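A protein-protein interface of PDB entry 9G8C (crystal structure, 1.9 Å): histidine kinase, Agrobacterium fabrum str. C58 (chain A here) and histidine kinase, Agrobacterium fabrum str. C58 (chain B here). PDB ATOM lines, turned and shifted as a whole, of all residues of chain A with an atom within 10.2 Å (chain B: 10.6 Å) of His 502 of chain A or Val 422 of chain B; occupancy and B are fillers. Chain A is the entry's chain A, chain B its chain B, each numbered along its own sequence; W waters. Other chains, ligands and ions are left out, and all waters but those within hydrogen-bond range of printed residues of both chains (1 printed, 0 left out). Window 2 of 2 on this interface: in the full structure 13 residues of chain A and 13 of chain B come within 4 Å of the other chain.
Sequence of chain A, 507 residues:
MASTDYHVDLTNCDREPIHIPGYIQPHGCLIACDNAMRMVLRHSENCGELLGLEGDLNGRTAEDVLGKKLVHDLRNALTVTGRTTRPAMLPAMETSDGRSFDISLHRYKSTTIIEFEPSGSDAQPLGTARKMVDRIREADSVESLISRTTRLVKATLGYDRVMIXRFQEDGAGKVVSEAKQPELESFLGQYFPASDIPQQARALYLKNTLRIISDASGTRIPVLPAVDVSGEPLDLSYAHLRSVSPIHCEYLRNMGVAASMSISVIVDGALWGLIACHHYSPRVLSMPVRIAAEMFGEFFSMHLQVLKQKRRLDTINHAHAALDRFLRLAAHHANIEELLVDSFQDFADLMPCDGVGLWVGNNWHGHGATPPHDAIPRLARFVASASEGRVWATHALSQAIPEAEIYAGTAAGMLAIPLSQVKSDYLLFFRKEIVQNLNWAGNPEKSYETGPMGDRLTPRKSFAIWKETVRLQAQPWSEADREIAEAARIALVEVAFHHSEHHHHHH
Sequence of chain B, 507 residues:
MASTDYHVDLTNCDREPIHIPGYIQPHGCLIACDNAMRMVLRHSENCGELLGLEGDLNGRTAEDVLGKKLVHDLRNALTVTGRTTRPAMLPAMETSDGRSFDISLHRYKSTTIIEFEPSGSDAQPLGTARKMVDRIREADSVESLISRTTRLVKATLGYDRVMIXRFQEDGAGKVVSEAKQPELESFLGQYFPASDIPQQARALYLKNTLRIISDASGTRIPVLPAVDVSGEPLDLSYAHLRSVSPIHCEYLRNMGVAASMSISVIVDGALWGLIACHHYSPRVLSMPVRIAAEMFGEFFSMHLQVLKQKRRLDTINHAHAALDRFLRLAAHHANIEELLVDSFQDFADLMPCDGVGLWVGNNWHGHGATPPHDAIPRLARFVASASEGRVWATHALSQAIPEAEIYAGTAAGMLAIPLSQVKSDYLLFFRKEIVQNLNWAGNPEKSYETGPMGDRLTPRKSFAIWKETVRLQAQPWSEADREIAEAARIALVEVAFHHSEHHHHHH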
ATOM      1  N   LEU A 327      18.090  38.321   2.302  1.00  0.00           N
ATOM      2  CA  LEU A 327      17.527  37.105   2.958  1.00  0.00           C
ATOM      3  C   LEU A 327      18.541  36.516   3.947  1.00  0.00           C
ATOM      4  O   LEU A 327      18.140  36.201   5.095  1.00  0.00           O
ATOM      5  CB  LEU A 327      17.130  36.085   1.890  1.00  0.00           C
ATOM      6  CG  LEU A 327      15.656  36.104   1.504  1.00  0.00           C
ATOM      7  CD1 LEU A 327      15.412  35.304   0.226  1.00  0.00           C
ATOM      8  CD2 LEU A 327      14.804  35.552   2.630  1.00  0.00           C
ATOM      9  N   ALA A 330      19.080  38.925   6.955  1.00  0.00           N
ATOM     10  CA  ALA A 330      17.873  38.986   7.808  1.00  0.00           C
ATOM     11  C   ALA A 330      17.821  37.790   8.777  1.00  0.00           C
ATOM     12  O   ALA A 330      17.241  37.935   9.868  1.00  0.00           O
ATOM     13  CB  ALA A 330      16.652  39.039   6.936  1.00  0.00           C
ATOM     14  N   ALA A 331      18.379  36.646   8.383  1.00  0.00           N
ATOM     15  CA  ALA A 331      18.281  35.374   9.138  1.00  0.00           C
ATOM     16  C   ALA A 331      18.936  35.527  10.520  1.00  0.00           C
ATOM     17  O   ALA A 331      18.478  34.843  11.442  1.00  0.00           O
ATOM     18  CB  ALA A 331      18.896  34.246   8.348  1.00  0.00           C
ATOM     19  N   HIS A 332      19.931  36.410  10.674  1.00  0.00           N
ATOM     20  CA  HIS A 332      20.619  36.640  11.974  1.00  0.00           C
ATOM     21  C   HIS A 332      20.200  37.976  12.605  1.00  0.00           C
ATOM     22  O   HIS A 332      20.971  38.489  13.434  1.00  0.00           O
ATOM     23  CB  HIS A 332      22.141  36.457  11.835  1.00  0.00           C
ATOM     24  CG  HIS A 332      22.850  37.418  10.941  1.00  0.00           C
ATOM     25  ND1 HIS A 332      23.339  37.044   9.700  1.00  0.00           N
ATOM     26  CD2 HIS A 332      23.225  38.704  11.123  1.00  0.00           C
ATOM     27  CE1 HIS A 332      23.961  38.069   9.146  1.00  0.00           C
ATOM     28  NE2 HIS A 332      23.911  39.102  10.002  1.00  0.00           N
ATOM     29  N   HIS A 333      19.005  38.485  12.282  1.00  0.00           N
ATOM     30  CA  HIS A 333      18.407  39.703  12.898  1.00  0.00           C
ATOM     31  C   HIS A 333      17.123  39.335  13.645  1.00  0.00           C
ATOM     32  O   HIS A 333      16.260  38.680  13.052  1.00  0.00           O
ATOM     33  CB  HIS A 333      18.153  40.800  11.851  1.00  0.00           C
ATOM     34  CG  HIS A 333      19.316  41.715  11.667  1.00  0.00           C
ATOM     35  ND1 HIS A 333      20.327  41.441  10.783  1.00  0.00           N
ATOM     36  CD2 HIS A 333      19.638  42.882  12.258  1.00  0.00           C
ATOM     37  CE1 HIS A 333      21.227  42.395  10.835  1.00  0.00           C
ATOM     38  NE2 HIS A 333      20.831  43.294  11.734  1.00  0.00           N
ATOM     39  N   ALA A 334      17.000  39.795  14.890  1.00  0.00           N
ATOM     40  CA  ALA A 334      15.843  39.543  15.780  1.00  0.00           C
ATOM     41  C   ALA A 334      14.740  40.564  15.497  1.00  0.00           C
ATOM     42  O   ALA A 334      13.563  40.243  15.714  1.00  0.00           O
ATOM     43  CB  ALA A 334      16.290  39.606  17.220  1.00  0.00           C
ATOM     44  N   ILE A 336      13.220  42.704  12.562  1.00  0.00           N
ATOM     45  CA  ILE A 336      13.129  42.860  11.078  1.00  0.00           C
ATOM     46  C   ILE A 336      12.745  44.304  10.738  1.00  0.00           C
ATOM     47  O   ILE A 336      13.283  44.830   9.748  1.00  0.00           O
ATOM     48  CB  ILE A 336      12.152  41.832  10.466  1.00  0.00           C
ATOM     49  CG1 ILE A 336      12.652  40.400  10.675  1.00  0.00           C
ATOM     50  CG2 ILE A 336      11.900  42.120   8.991  1.00  0.00           C
ATOM     51  CD1 ILE A 336      14.043  40.150  10.145  1.00  0.00           C
ATOM     52  N   GLU A 494       9.290  35.851   2.537  1.00  0.00           N
ATOM     53  CA  GLU A 494      10.223  34.811   3.041  1.00  0.00           C
ATOM     54  C   GLU A 494      10.894  35.287   4.335  1.00  0.00           C
ATOM     55  O   GLU A 494      10.990  34.473   5.276  1.00  0.00           O
ATOM     56  CB  GLU A 494      11.320  34.478   2.043  1.00  0.00           C
ATOM     57  CG  GLU A 494      10.976  33.364   1.091  1.00  0.00           C
ATOM     58  CD  GLU A 494      12.193  32.561   0.674  1.00  0.00           C
ATOM     59  OE1 GLU A 494      12.667  32.807  -0.425  1.00  0.00           O
ATOM     60  OE2 GLU A 494      12.676  31.723   1.469  1.00  0.00           O
ATOM     61  N   VAL A 495      11.390  36.526   4.370  1.00  0.00           N
ATOM     62  CA  VAL A 495      12.026  37.082   5.604  1.00  0.00           C
ATOM     63  C   VAL A 495      11.021  36.974   6.753  1.00  0.00           C
ATOM     64  O   VAL A 495      11.375  36.404   7.784  1.00  0.00           O
ATOM     65  CB  VAL A 495      12.517  38.526   5.393  1.00  0.00           C
ATOM     66  CG1 VAL A 495      12.851  39.216   6.711  1.00  0.00           C
ATOM     67  CG2 VAL A 495      13.711  38.549   4.461  1.00  0.00           C
ATOM     68  N   ALA A 496       9.806  37.472   6.553  1.00  0.00           N
ATOM     69  CA  ALA A 496       8.730  37.520   7.566  1.00  0.00           C
ATOM     70  C   ALA A 496       8.397  36.100   8.049  1.00  0.00           C
ATOM     71  O   ALA A 496       8.305  35.908   9.278  1.00  0.00           O
ATOM     72  CB  ALA A 496       7.525  38.209   6.995  1.00  0.00           C
ATOM     73  N   PHE A 497       8.258  35.130   7.134  1.00  0.00           N
ATOM     74  CA  PHE A 497       7.854  33.741   7.476  1.00  0.00           C
ATOM     75  C   PHE A 497       8.956  33.042   8.271  1.00  0.00           C
ATOM     76  O   PHE A 497       8.632  32.456   9.328  1.00  0.00           O
ATOM     77  CB  PHE A 497       7.505  32.898   6.245  1.00  0.00           C
ATOM     78  CG  PHE A 497       6.960  31.533   6.599  1.00  0.00           C
ATOM     79  CD1 PHE A 497       5.800  31.411   7.353  1.00  0.00           C
ATOM     80  CD2 PHE A 497       7.620  30.374   6.216  1.00  0.00           C
ATOM     81  CE1 PHE A 497       5.302  30.159   7.695  1.00  0.00           C
ATOM     82  CE2 PHE A 497       7.117  29.124   6.555  1.00  0.00           C
ATOM     83  CZ  PHE A 497       5.960  29.021   7.292  1.00  0.00           C
ATOM     84  N   HIS A 498      10.201  33.074   7.788  1.00  0.00           N
ATOM     85  CA  HIS A 498      11.322  32.353   8.442  1.00  0.00           C
ATOM     86  C   HIS A 498      11.534  32.971   9.825  1.00  0.00           C
ATOM     87  O   HIS A 498      11.860  32.227  10.765  1.00  0.00           O
ATOM     88  CB  HIS A 498      12.583  32.331   7.574  1.00  0.00           C
ATOM     89  CG  HIS A 498      12.387  31.691   6.238  1.00  0.00           C
ATOM     90  ND1 HIS A 498      11.706  30.494   6.070  1.00  0.00           N
ATOM     91  CD2 HIS A 498      12.789  32.072   5.004  1.00  0.00           C
ATOM     92  CE1 HIS A 498      11.689  30.177   4.787  1.00  0.00           C
ATOM     93  NE2 HIS A 498      12.337  31.140   4.113  1.00  0.00           N
ATOM     94  N   HIS A 499      11.305  34.282   9.943  1.00  0.00           N
ATOM     95  CA  HIS A 499      11.406  35.011  11.233  1.00  0.00           C
ATOM     96  C   HIS A 499      10.410  34.412  12.234  1.00  0.00           C
ATOM     97  O   HIS A 499      10.842  34.095  13.350  1.00  0.00           O
ATOM     98  CB  HIS A 499      11.205  36.512  11.038  1.00  0.00           C
ATOM     99  CG  HIS A 499      11.477  37.270  12.286  1.00  0.00           C
ATOM    100  ND1 HIS A 499      12.763  37.443  12.758  1.00  0.00           N
ATOM    101  CD2 HIS A 499      10.642  37.851  13.178  1.00  0.00           C
ATOM    102  CE1 HIS A 499      12.711  38.124  13.884  1.00  0.00           C
ATOM    103  NE2 HIS A 499      11.415  38.388  14.165  1.00  0.00           N
ATOM    104  N   SER A 500       9.142  34.249  11.848  1.00  0.00           N
ATOM    105  CA  SER A 500       8.091  33.674  12.733  1.00  0.00           C
ATOM    106  C   SER A 500       8.439  32.210  13.042  1.00  0.00           C
ATOM    107  O   SER A 500       8.311  31.812  14.218  1.00  0.00           O
ATOM    108  CB  SER A 500       6.716  33.810  12.151  1.00  0.00           C
ATOM    109  OG  SER A 500       6.572  32.979  11.012  1.00  0.00           O
ATOM    110  N   GLU A 501       8.910  31.455  12.041  1.00  0.00           N
ATOM    111  CA  GLU A 501       9.352  30.042  12.202  1.00  0.00           C
ATOM    112  C   GLU A 501      10.334  29.929  13.375  1.00  0.00           C
ATOM    113  O   GLU A 501      10.225  28.937  14.113  1.00  0.00           O
ATOM    114  CB  GLU A 501      10.002  29.490  10.927  1.00  0.00           C
ATOM    115  CG  GLU A 501       9.008  28.982   9.896  1.00  0.00           C
ATOM    116  CD  GLU A 501       9.646  28.381   8.652  1.00  0.00           C
ATOM    117  OE1 GLU A 501      10.475  29.074   8.030  1.00  0.00           O
ATOM    118  OE2 GLU A 501       9.324  27.217   8.315  1.00  0.00           O
ATOM    119  N   HIS A 502      11.264  30.880  13.533  1.00  0.00           N
ATOM    120  CA  HIS A 502      12.390  30.780  14.504  1.00  0.00           C
ATOM    121  C   HIS A 502      12.224  31.744  15.693  1.00  0.00           C
ATOM    122  O   HIS A 502      13.172  31.823  16.499  1.00  0.00           O
ATOM    123  CB  HIS A 502      13.732  31.005  13.796  1.00  0.00           C
ATOM    124  CG  HIS A 502      13.982  30.121  12.619  1.00  0.00           C
ATOM    125  ND1 HIS A 502      14.146  28.750  12.735  1.00  0.00           N
ATOM    126  CD2 HIS A 502      14.150  30.410  11.309  1.00  0.00           C
ATOM    127  CE1 HIS A 502      14.380  28.234  11.544  1.00  0.00           C
ATOM    128  NE2 HIS A 502      14.383  29.232  10.649  1.00  0.00           N
ATOM    129  N   HIS A 503      11.089  32.446  15.815  1.00  0.00           N
ATOM    130  CA  HIS A 503      10.839  33.478  16.866  1.00  0.00           C
ATOM    131  C   HIS A 503       9.356  33.484  17.249  1.00  0.00           C
ATOM    132  O   HIS A 503       8.814  32.452  17.635  1.00  0.00           O
ATOM    133  CB  HIS A 503      11.267  34.884  16.405  1.00  0.00           C
ATOM    134  CG  HIS A 503      12.732  35.073  16.169  1.00  0.00           C
ATOM    135  ND1 HIS A 503      13.344  34.719  14.977  1.00  0.00           N
ATOM    136  CD2 HIS A 503      13.697  35.622  16.939  1.00  0.00           C
ATOM    137  CE1 HIS A 503      14.625  35.024  15.033  1.00  0.00           C
ATOM    138  NE2 HIS A 503      14.870  35.579  16.227  1.00  0.00           N
ATOM    139  N   GLY B 361       4.620  15.308   8.549  1.00  0.00           N
ATOM    140  CA  GLY B 361       4.340  14.795   9.906  1.00  0.00           C
ATOM    141  C   GLY B 361       4.551  13.291   9.999  1.00  0.00           C
ATOM    142  O   GLY B 361       3.727  12.621  10.652  1.00  0.00           O
ATOM    143  N   ASN B 362       5.613  12.776   9.370  1.00  0.00           N
ATOM    144  CA  ASN B 362       5.969  11.335   9.383  1.00  0.00           C
ATOM    145  C   ASN B 362       4.894  10.495   8.677  1.00  0.00           C
ATOM    146  O   ASN B 362       4.876   9.272   8.924  1.00  0.00           O
ATOM    147  CB  ASN B 362       6.155  10.780  10.796  1.00  0.00           C
ATOM    148  CG  ASN B 362       7.211  11.523  11.580  1.00  0.00           C
ATOM    149  OD1 ASN B 362       6.916  12.147  12.600  1.00  0.00           O
ATOM    150  ND2 ASN B 362       8.439  11.451  11.109  1.00  0.00           N
ATOM    151  N   ALA B 384      17.539  16.518   5.259  1.00  0.00           N
ATOM    152  CA  ALA B 384      17.558  17.423   6.437  1.00  0.00           C
ATOM    153  C   ALA B 384      19.009  17.758   6.824  1.00  0.00           C
ATOM    154  O   ALA B 384      19.322  18.949   7.037  1.00  0.00           O
ATOM    155  CB  ALA B 384      16.810  16.779   7.577  1.00  0.00           C
ATOM    156  N   SER B 387      20.934  19.601   3.347  1.00  0.00           N
ATOM    157  CA  SER B 387      20.470  20.891   2.767  1.00  0.00           C
ATOM    158  C   SER B 387      20.430  21.979   3.849  1.00  0.00           C
ATOM    159  O   SER B 387      20.298  21.632   5.037  1.00  0.00           O
ATOM    160  CB  SER B 387      19.133  20.738   2.093  1.00  0.00           C
ATOM    161  OG  SER B 387      18.168  20.207   2.988  1.00  0.00           O
ATOM    162  N   GLU B 388      20.534  23.236   3.415  1.00  0.00           N
ATOM    163  CA  GLU B 388      20.457  24.450   4.270  1.00  0.00           C
ATOM    164  C   GLU B 388      19.083  25.093   4.067  1.00  0.00           C
ATOM    165  O   GLU B 388      19.022  26.335   3.935  1.00  0.00           O
ATOM    166  CB  GLU B 388      21.587  25.419   3.914  1.00  0.00           C
ATOM    167  N   GLY B 389      18.025  24.275   4.032  1.00  0.00           N
ATOM    168  CA  GLY B 389      16.631  24.741   3.882  1.00  0.00           C
ATOM    169  C   GLY B 389      16.338  25.256   2.484  1.00  0.00           C
ATOM    170  O   GLY B 389      15.369  26.012   2.338  1.00  0.00           O
ATOM    171  N   ARG B 390      17.134  24.870   1.480  1.00  0.00           N
ATOM    172  CA  ARG B 390      16.774  25.105   0.056  1.00  0.00           C
ATOM    173  C   ARG B 390      16.594  23.750  -0.654  1.00  0.00           C
ATOM    174  O   ARG B 390      16.732  22.694  -0.020  1.00  0.00           O
ATOM    175  CB  ARG B 390      17.825  25.989  -0.625  1.00  0.00           C
ATOM    176  N   PRO B 418      11.906  21.547   0.503  1.00  0.00           N
ATOM    177  CA  PRO B 418      11.525  21.709   1.906  1.00  0.00           C
ATOM    178  C   PRO B 418      10.191  22.453   2.030  1.00  0.00           C
ATOM    179  O   PRO B 418      10.007  23.448   1.338  1.00  0.00           O
ATOM    180  CB  PRO B 418      12.626  22.580   2.552  1.00  0.00           C
ATOM    181  CG  PRO B 418      13.675  22.784   1.480  1.00  0.00           C
ATOM    182  CD  PRO B 418      13.081  22.359   0.147  1.00  0.00           C
ATOM    183  N   LEU B 419       9.317  21.988   2.924  1.00  0.00           N
ATOM    184  CA  LEU B 419       8.004  22.623   3.210  1.00  0.00           C
ATOM    185  C   LEU B 419       8.067  23.431   4.515  1.00  0.00           C
ATOM    186  O   LEU B 419       7.059  24.082   4.855  1.00  0.00           O
ATOM    187  CB  LEU B 419       6.924  21.538   3.293  1.00  0.00           C
ATOM    188  CG  LEU B 419       6.855  20.542   2.131  1.00  0.00           C
ATOM    189  CD1 LEU B 419       5.708  19.579   2.323  1.00  0.00           C
ATOM    190  CD2 LEU B 419       6.700  21.223   0.786  1.00  0.00           C
ATOM    191  N   SER B 420       9.194  23.392   5.228  1.00  0.00           N
ATOM    192  CA  SER B 420       9.362  24.072   6.540  1.00  0.00           C
ATOM    193  C   SER B 420      10.847  24.188   6.885  1.00  0.00           C
ATOM    194  O   SER B 420      11.619  23.318   6.431  1.00  0.00           O
ATOM    195  CB  SER B 420       8.630  23.330   7.628  1.00  0.00           C
ATOM    196  OG  SER B 420       9.134  23.707   8.898  1.00  0.00           O
ATOM    197  N   GLN B 421      11.212  25.204   7.669  1.00  0.00           N
ATOM    198  CA  GLN B 421      12.591  25.341   8.207  1.00  0.00           C
ATOM    199  C   GLN B 421      12.659  24.703   9.607  1.00  0.00           C
ATOM    200  O   GLN B 421      13.782  24.592  10.120  1.00  0.00           O
ATOM    201  CB  GLN B 421      13.052  26.803   8.186  1.00  0.00           C
ATOM    202  CG  GLN B 421      13.635  27.236   6.843  1.00  0.00           C
ATOM    203  CD  GLN B 421      14.209  28.636   6.848  1.00  0.00           C
ATOM    204  OE1 GLN B 421      14.376  29.270   7.885  1.00  0.00           O
ATOM    205  NE2 GLN B 421      14.524  29.139   5.666  1.00  0.00           N
ATOM    206  N   VAL B 422      11.537  24.251  10.179  1.00  0.00           N
ATOM    207  CA  VAL B 422      11.495  23.744  11.588  1.00  0.00           C
ATOM    208  C   VAL B 422      10.989  22.296  11.673  1.00  0.00           C
ATOM    209  O   VAL B 422      11.058  21.749  12.781  1.00  0.00           O
ATOM    210  CB  VAL B 422      10.673  24.679  12.494  1.00  0.00           C
ATOM    211  CG1 VAL B 422      11.298  26.067  12.541  1.00  0.00           C
ATOM    212  CG2 VAL B 422       9.216  24.769  12.077  1.00  0.00           C
ATOM    213  N   LYS B 423      10.490  21.703  10.580  1.00  0.00           N
ATOM    214  CA  LYS B 423      10.072  20.269  10.519  1.00  0.00           C
ATOM    215  C   LYS B 423      10.662  19.663   9.242  1.00  0.00           C
ATOM    216  O   LYS B 423      10.778  20.408   8.240  1.00  0.00           O
ATOM    217  CB  LYS B 423       8.545  20.151  10.562  1.00  0.00           C
ATOM    218  N   SER B 424      11.041  18.382   9.253  1.00  0.00           N
ATOM    219  CA  SER B 424      11.623  17.723   8.049  1.00  0.00           C
ATOM    220  C   SER B 424      10.477  17.183   7.176  1.00  0.00           C
ATOM    221  O   SER B 424      10.323  15.940   7.041  1.00  0.00           O
ATOM    222  CB  SER B 424      12.653  16.695   8.401  1.00  0.00           C
ATOM    223  OG  SER B 424      12.131  15.762   9.321  1.00  0.00           O
ATOM    224  N   ASP B 425       9.693  18.116   6.631  1.00  0.00           N
ATOM    225  CA  ASP B 425       8.534  17.886   5.732  1.00  0.00           C
ATOM    226  C   ASP B 425       8.956  18.274   4.304  1.00  0.00           C
ATOM    227  O   ASP B 425       9.544  19.364   4.133  1.00  0.00           O
ATOM    228  CB  ASP B 425       7.322  18.702   6.183  1.00  0.00           C
ATOM    229  CG  ASP B 425       6.696  18.283   7.514  1.00  0.00           C
ATOM    230  OD1 ASP B 425       7.011  17.180   8.002  1.00  0.00           O
ATOM    231  OD2 ASP B 425       5.885  19.069   8.040  1.00  0.00           O
ATOM    232  N   TYR B 426       8.678  17.425   3.309  1.00  0.00           N
ATOM    233  CA  TYR B 426       9.180  17.612   1.922  1.00  0.00           C
ATOM    234  C   TYR B 426       8.117  17.231   0.906  1.00  0.00           C
ATOM    235  O   TYR B 426       7.294  16.316   1.170  1.00  0.00           O
ATOM    236  CB  TYR B 426      10.428  16.772   1.653  1.00  0.00           C
ATOM    237  CG  TYR B 426      11.580  17.117   2.556  1.00  0.00           C
ATOM    238  CD1 TYR B 426      12.353  18.235   2.308  1.00  0.00           C
ATOM    239  CD2 TYR B 426      11.853  16.370   3.686  1.00  0.00           C
ATOM    240  CE1 TYR B 426      13.397  18.587   3.139  1.00  0.00           C
ATOM    241  CE2 TYR B 426      12.898  16.708   4.531  1.00  0.00           C
ATOM    242  CZ  TYR B 426      13.666  17.825   4.257  1.00  0.00           C
ATOM    243  OH  TYR B 426      14.703  18.173   5.068  1.00  0.00           O
ATOM    244  N   ARG B 489       9.093  25.988  -4.058  1.00  0.00           N
ATOM    245  CA  ARG B 489       9.520  26.184  -2.645  1.00  0.00           C
ATOM    246  C   ARG B 489       8.956  27.516  -2.147  1.00  0.00           C
ATOM    247  O   ARG B 489       8.390  27.556  -1.046  1.00  0.00           O
ATOM    248  CB  ARG B 489      11.044  26.184  -2.506  1.00  0.00           C
ATOM    249  CG  ARG B 489      11.529  26.194  -1.061  1.00  0.00           C
ATOM    250  CD  ARG B 489      13.023  26.396  -0.937  1.00  0.00           C
ATOM    251  NE  ARG B 489      13.449  27.695  -1.449  1.00  0.00           N
ATOM    252  CZ  ARG B 489      13.368  28.856  -0.789  1.00  0.00           C
ATOM    253  NH1 ARG B 489      12.827  28.933   0.419  1.00  0.00           N
ATOM    254  NH2 ARG B 489      13.800  29.959  -1.365  1.00  0.00           N
ATOM    255  N   VAL B 493       6.130  28.609   0.791  1.00  0.00           N
ATOM    256  CA  VAL B 493       6.456  29.603   1.852  1.00  0.00           C
ATOM    257  C   VAL B 493       5.317  30.623   1.886  1.00  0.00           C
ATOM    258  O   VAL B 493       4.816  30.932   2.986  1.00  0.00           O
ATOM    259  CB  VAL B 493       7.810  30.291   1.630  1.00  0.00           C
ATOM    260  CG1 VAL B 493       7.948  31.509   2.536  1.00  0.00           C
ATOM    261  CG2 VAL B 493       8.968  29.330   1.848  1.00  0.00           C
ATOM    262  N   ALA B 496       2.021  29.240   3.262  1.00  0.00           N
ATOM    263  CA  ALA B 496       2.167  29.025   4.720  1.00  0.00           C
ATOM    264  C   ALA B 496       2.086  30.378   5.444  1.00  0.00           C
ATOM    265  O   ALA B 496       1.424  30.454   6.502  1.00  0.00           O
ATOM    266  CB  ALA B 496       3.449  28.296   5.028  1.00  0.00           C
ATOM    267  N   PHE B 497       2.739  31.411   4.905  1.00  0.00           N
ATOM    268  CA  PHE B 497       2.831  32.740   5.561  1.00  0.00           C
ATOM    269  C   PHE B 497       1.452  33.398   5.578  1.00  0.00           C
ATOM    270  O   PHE B 497       1.031  33.835   6.659  1.00  0.00           O
ATOM    271  CB  PHE B 497       3.858  33.662   4.897  1.00  0.00           C
ATOM    272  CG  PHE B 497       3.980  34.996   5.600  1.00  0.00           C
ATOM    273  CD1 PHE B 497       4.413  35.059   6.916  1.00  0.00           C
ATOM    274  CD2 PHE B 497       3.619  36.176   4.973  1.00  0.00           C
ATOM    275  CE1 PHE B 497       4.495  36.277   7.581  1.00  0.00           C
ATOM    276  CE2 PHE B 497       3.718  37.395   5.633  1.00  0.00           C
ATOM    277  CZ  PHE B 497       4.151  37.440   6.936  1.00  0.00           C
HETATM  278  O   HOH W   1       6.982  26.034   8.817  1.00  0.00           O
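The side-chain carboxylate of Glu 494 of chain A is in salt-bridge range of the guanidinium group of Arg 489 of chain B. A ring nitrogen (ND1) of His 498 of chain A lies close to the side-chain amide nitrogen of Gln 421 of chain B (3.2 Å). The backbone NH (N) of Gln 421 of chain B sits at hydrogen-bond distance from the side-chain carboxylate (OE2) of Glu 501 of chain A (2.8 Å). OE1 of Gln 421 of chain B lies within hydrogen-bond range of NE2 of His 502 of chain A (2.8 Å).
The side-chain carboxylate (OE2) of Glu 494 of chain A lies within hydrogen-bond range of a ring nitrogen (NE2) of His 498 of chain A (2.7 Å). The backbone carbonyl oxygen (O) of Phe 497 of chain A is in hydrogen-bond range of the side-chain hydroxyl (OG) of Ser 500 of chain A (2.7 Å). The side-chain carboxylate (OE1) of Glu 501 of chain A sits at hydrogen-bond distance from a ring nitrogen (ND1) of His 498 of chain A (2.7 Å). The side-chain hydroxyl of Ser 420 of chain B is in hydrogen-bond range of the backbone NH of Val 422 of chain B, at 2.8 Å. The side-chain hydroxyl (OG) of Ser 420 of chain B lies within hydrogen-bond range of the backbone NH (N) of Lys 423 of chain B (2.9 Å).
Among the printed residues, merely in contact across the chains: Glu 494 of chain A with Val 493 of chain B (3.8 Å), Ala 496 of chain A with Phe 497 of chain B (3.5 Å), Phe 497 of chain A with Val 493 of chain B (3.9 Å), Phe 497 of chain A with Ala 496 of chain B (3.5 Å), Phe 497 of chain A with Phe 497 of chain B (3.7 Å), Glu 501 of chain A with Ser 420 of chain B (3.6 Å), Glu 501 of chain A with Val 422 of chain B (3.4 Å) and His 502 of chain A with Val 422 of chain B (3.9 Å).
Ile 336 of chain A touches none of the printed residues of chain B. Of the printed residues of chain B, Glu 494 of chain A touches Arg 489 (3.0 Å) and Val 493 (3.8 Å). Printed residues of chain B within 4 Å of Ala 496 of chain A: Phe 497 (3.5 Å). No residue of chain B comes within 4 Å of Ser 500 of chain A. Of chain B, only Gln 421 and Val 422 come within 4 Å of His 502 of chain A. No residue of chain B comes within 4 Å of His 503 of chain A. No residue of chain A comes within 4 Å of Lys 423 of chain B. Asp 425 of chain B touches none of the printed residues of chain A. The nearest residue of chain A that does not touch Val 422 of chain B is His 498 of chain A (6.4 Å). The nearest printed residue of chain B that does not touch His 498 of chain A is Val 493 of chain B (4.1 Å).
Printed residues of chain B that touch a printed residue of chain A: Ser 420, Gln 421, Val 422, Arg 489, Val 493, Ala 496 and Phe 497. Hydrophobic or aromatic side chains of chain B within 4 Å of the printed part of chain A: Val 422, Val 493, Ala 496 and Phe 497. Of the 17 printed residues of chain A, 6 touch a printed residue of chain B. Along chain A the printed residues that touch a printed residue of chain B span positions 494 to 502. Among the printed residues, Asp or Glu carboxylates within 4 Å of a Lys or Arg side-chain nitrogen of the other chain: Glu 494 of chain A with Arg 489 of chain B (3.0 Å).
Water W1 bridges the side-chain carboxylate (OE2) of Glu 501 of chain A and the side-chain hydroxyl (OG) of Ser 420 of chain B.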
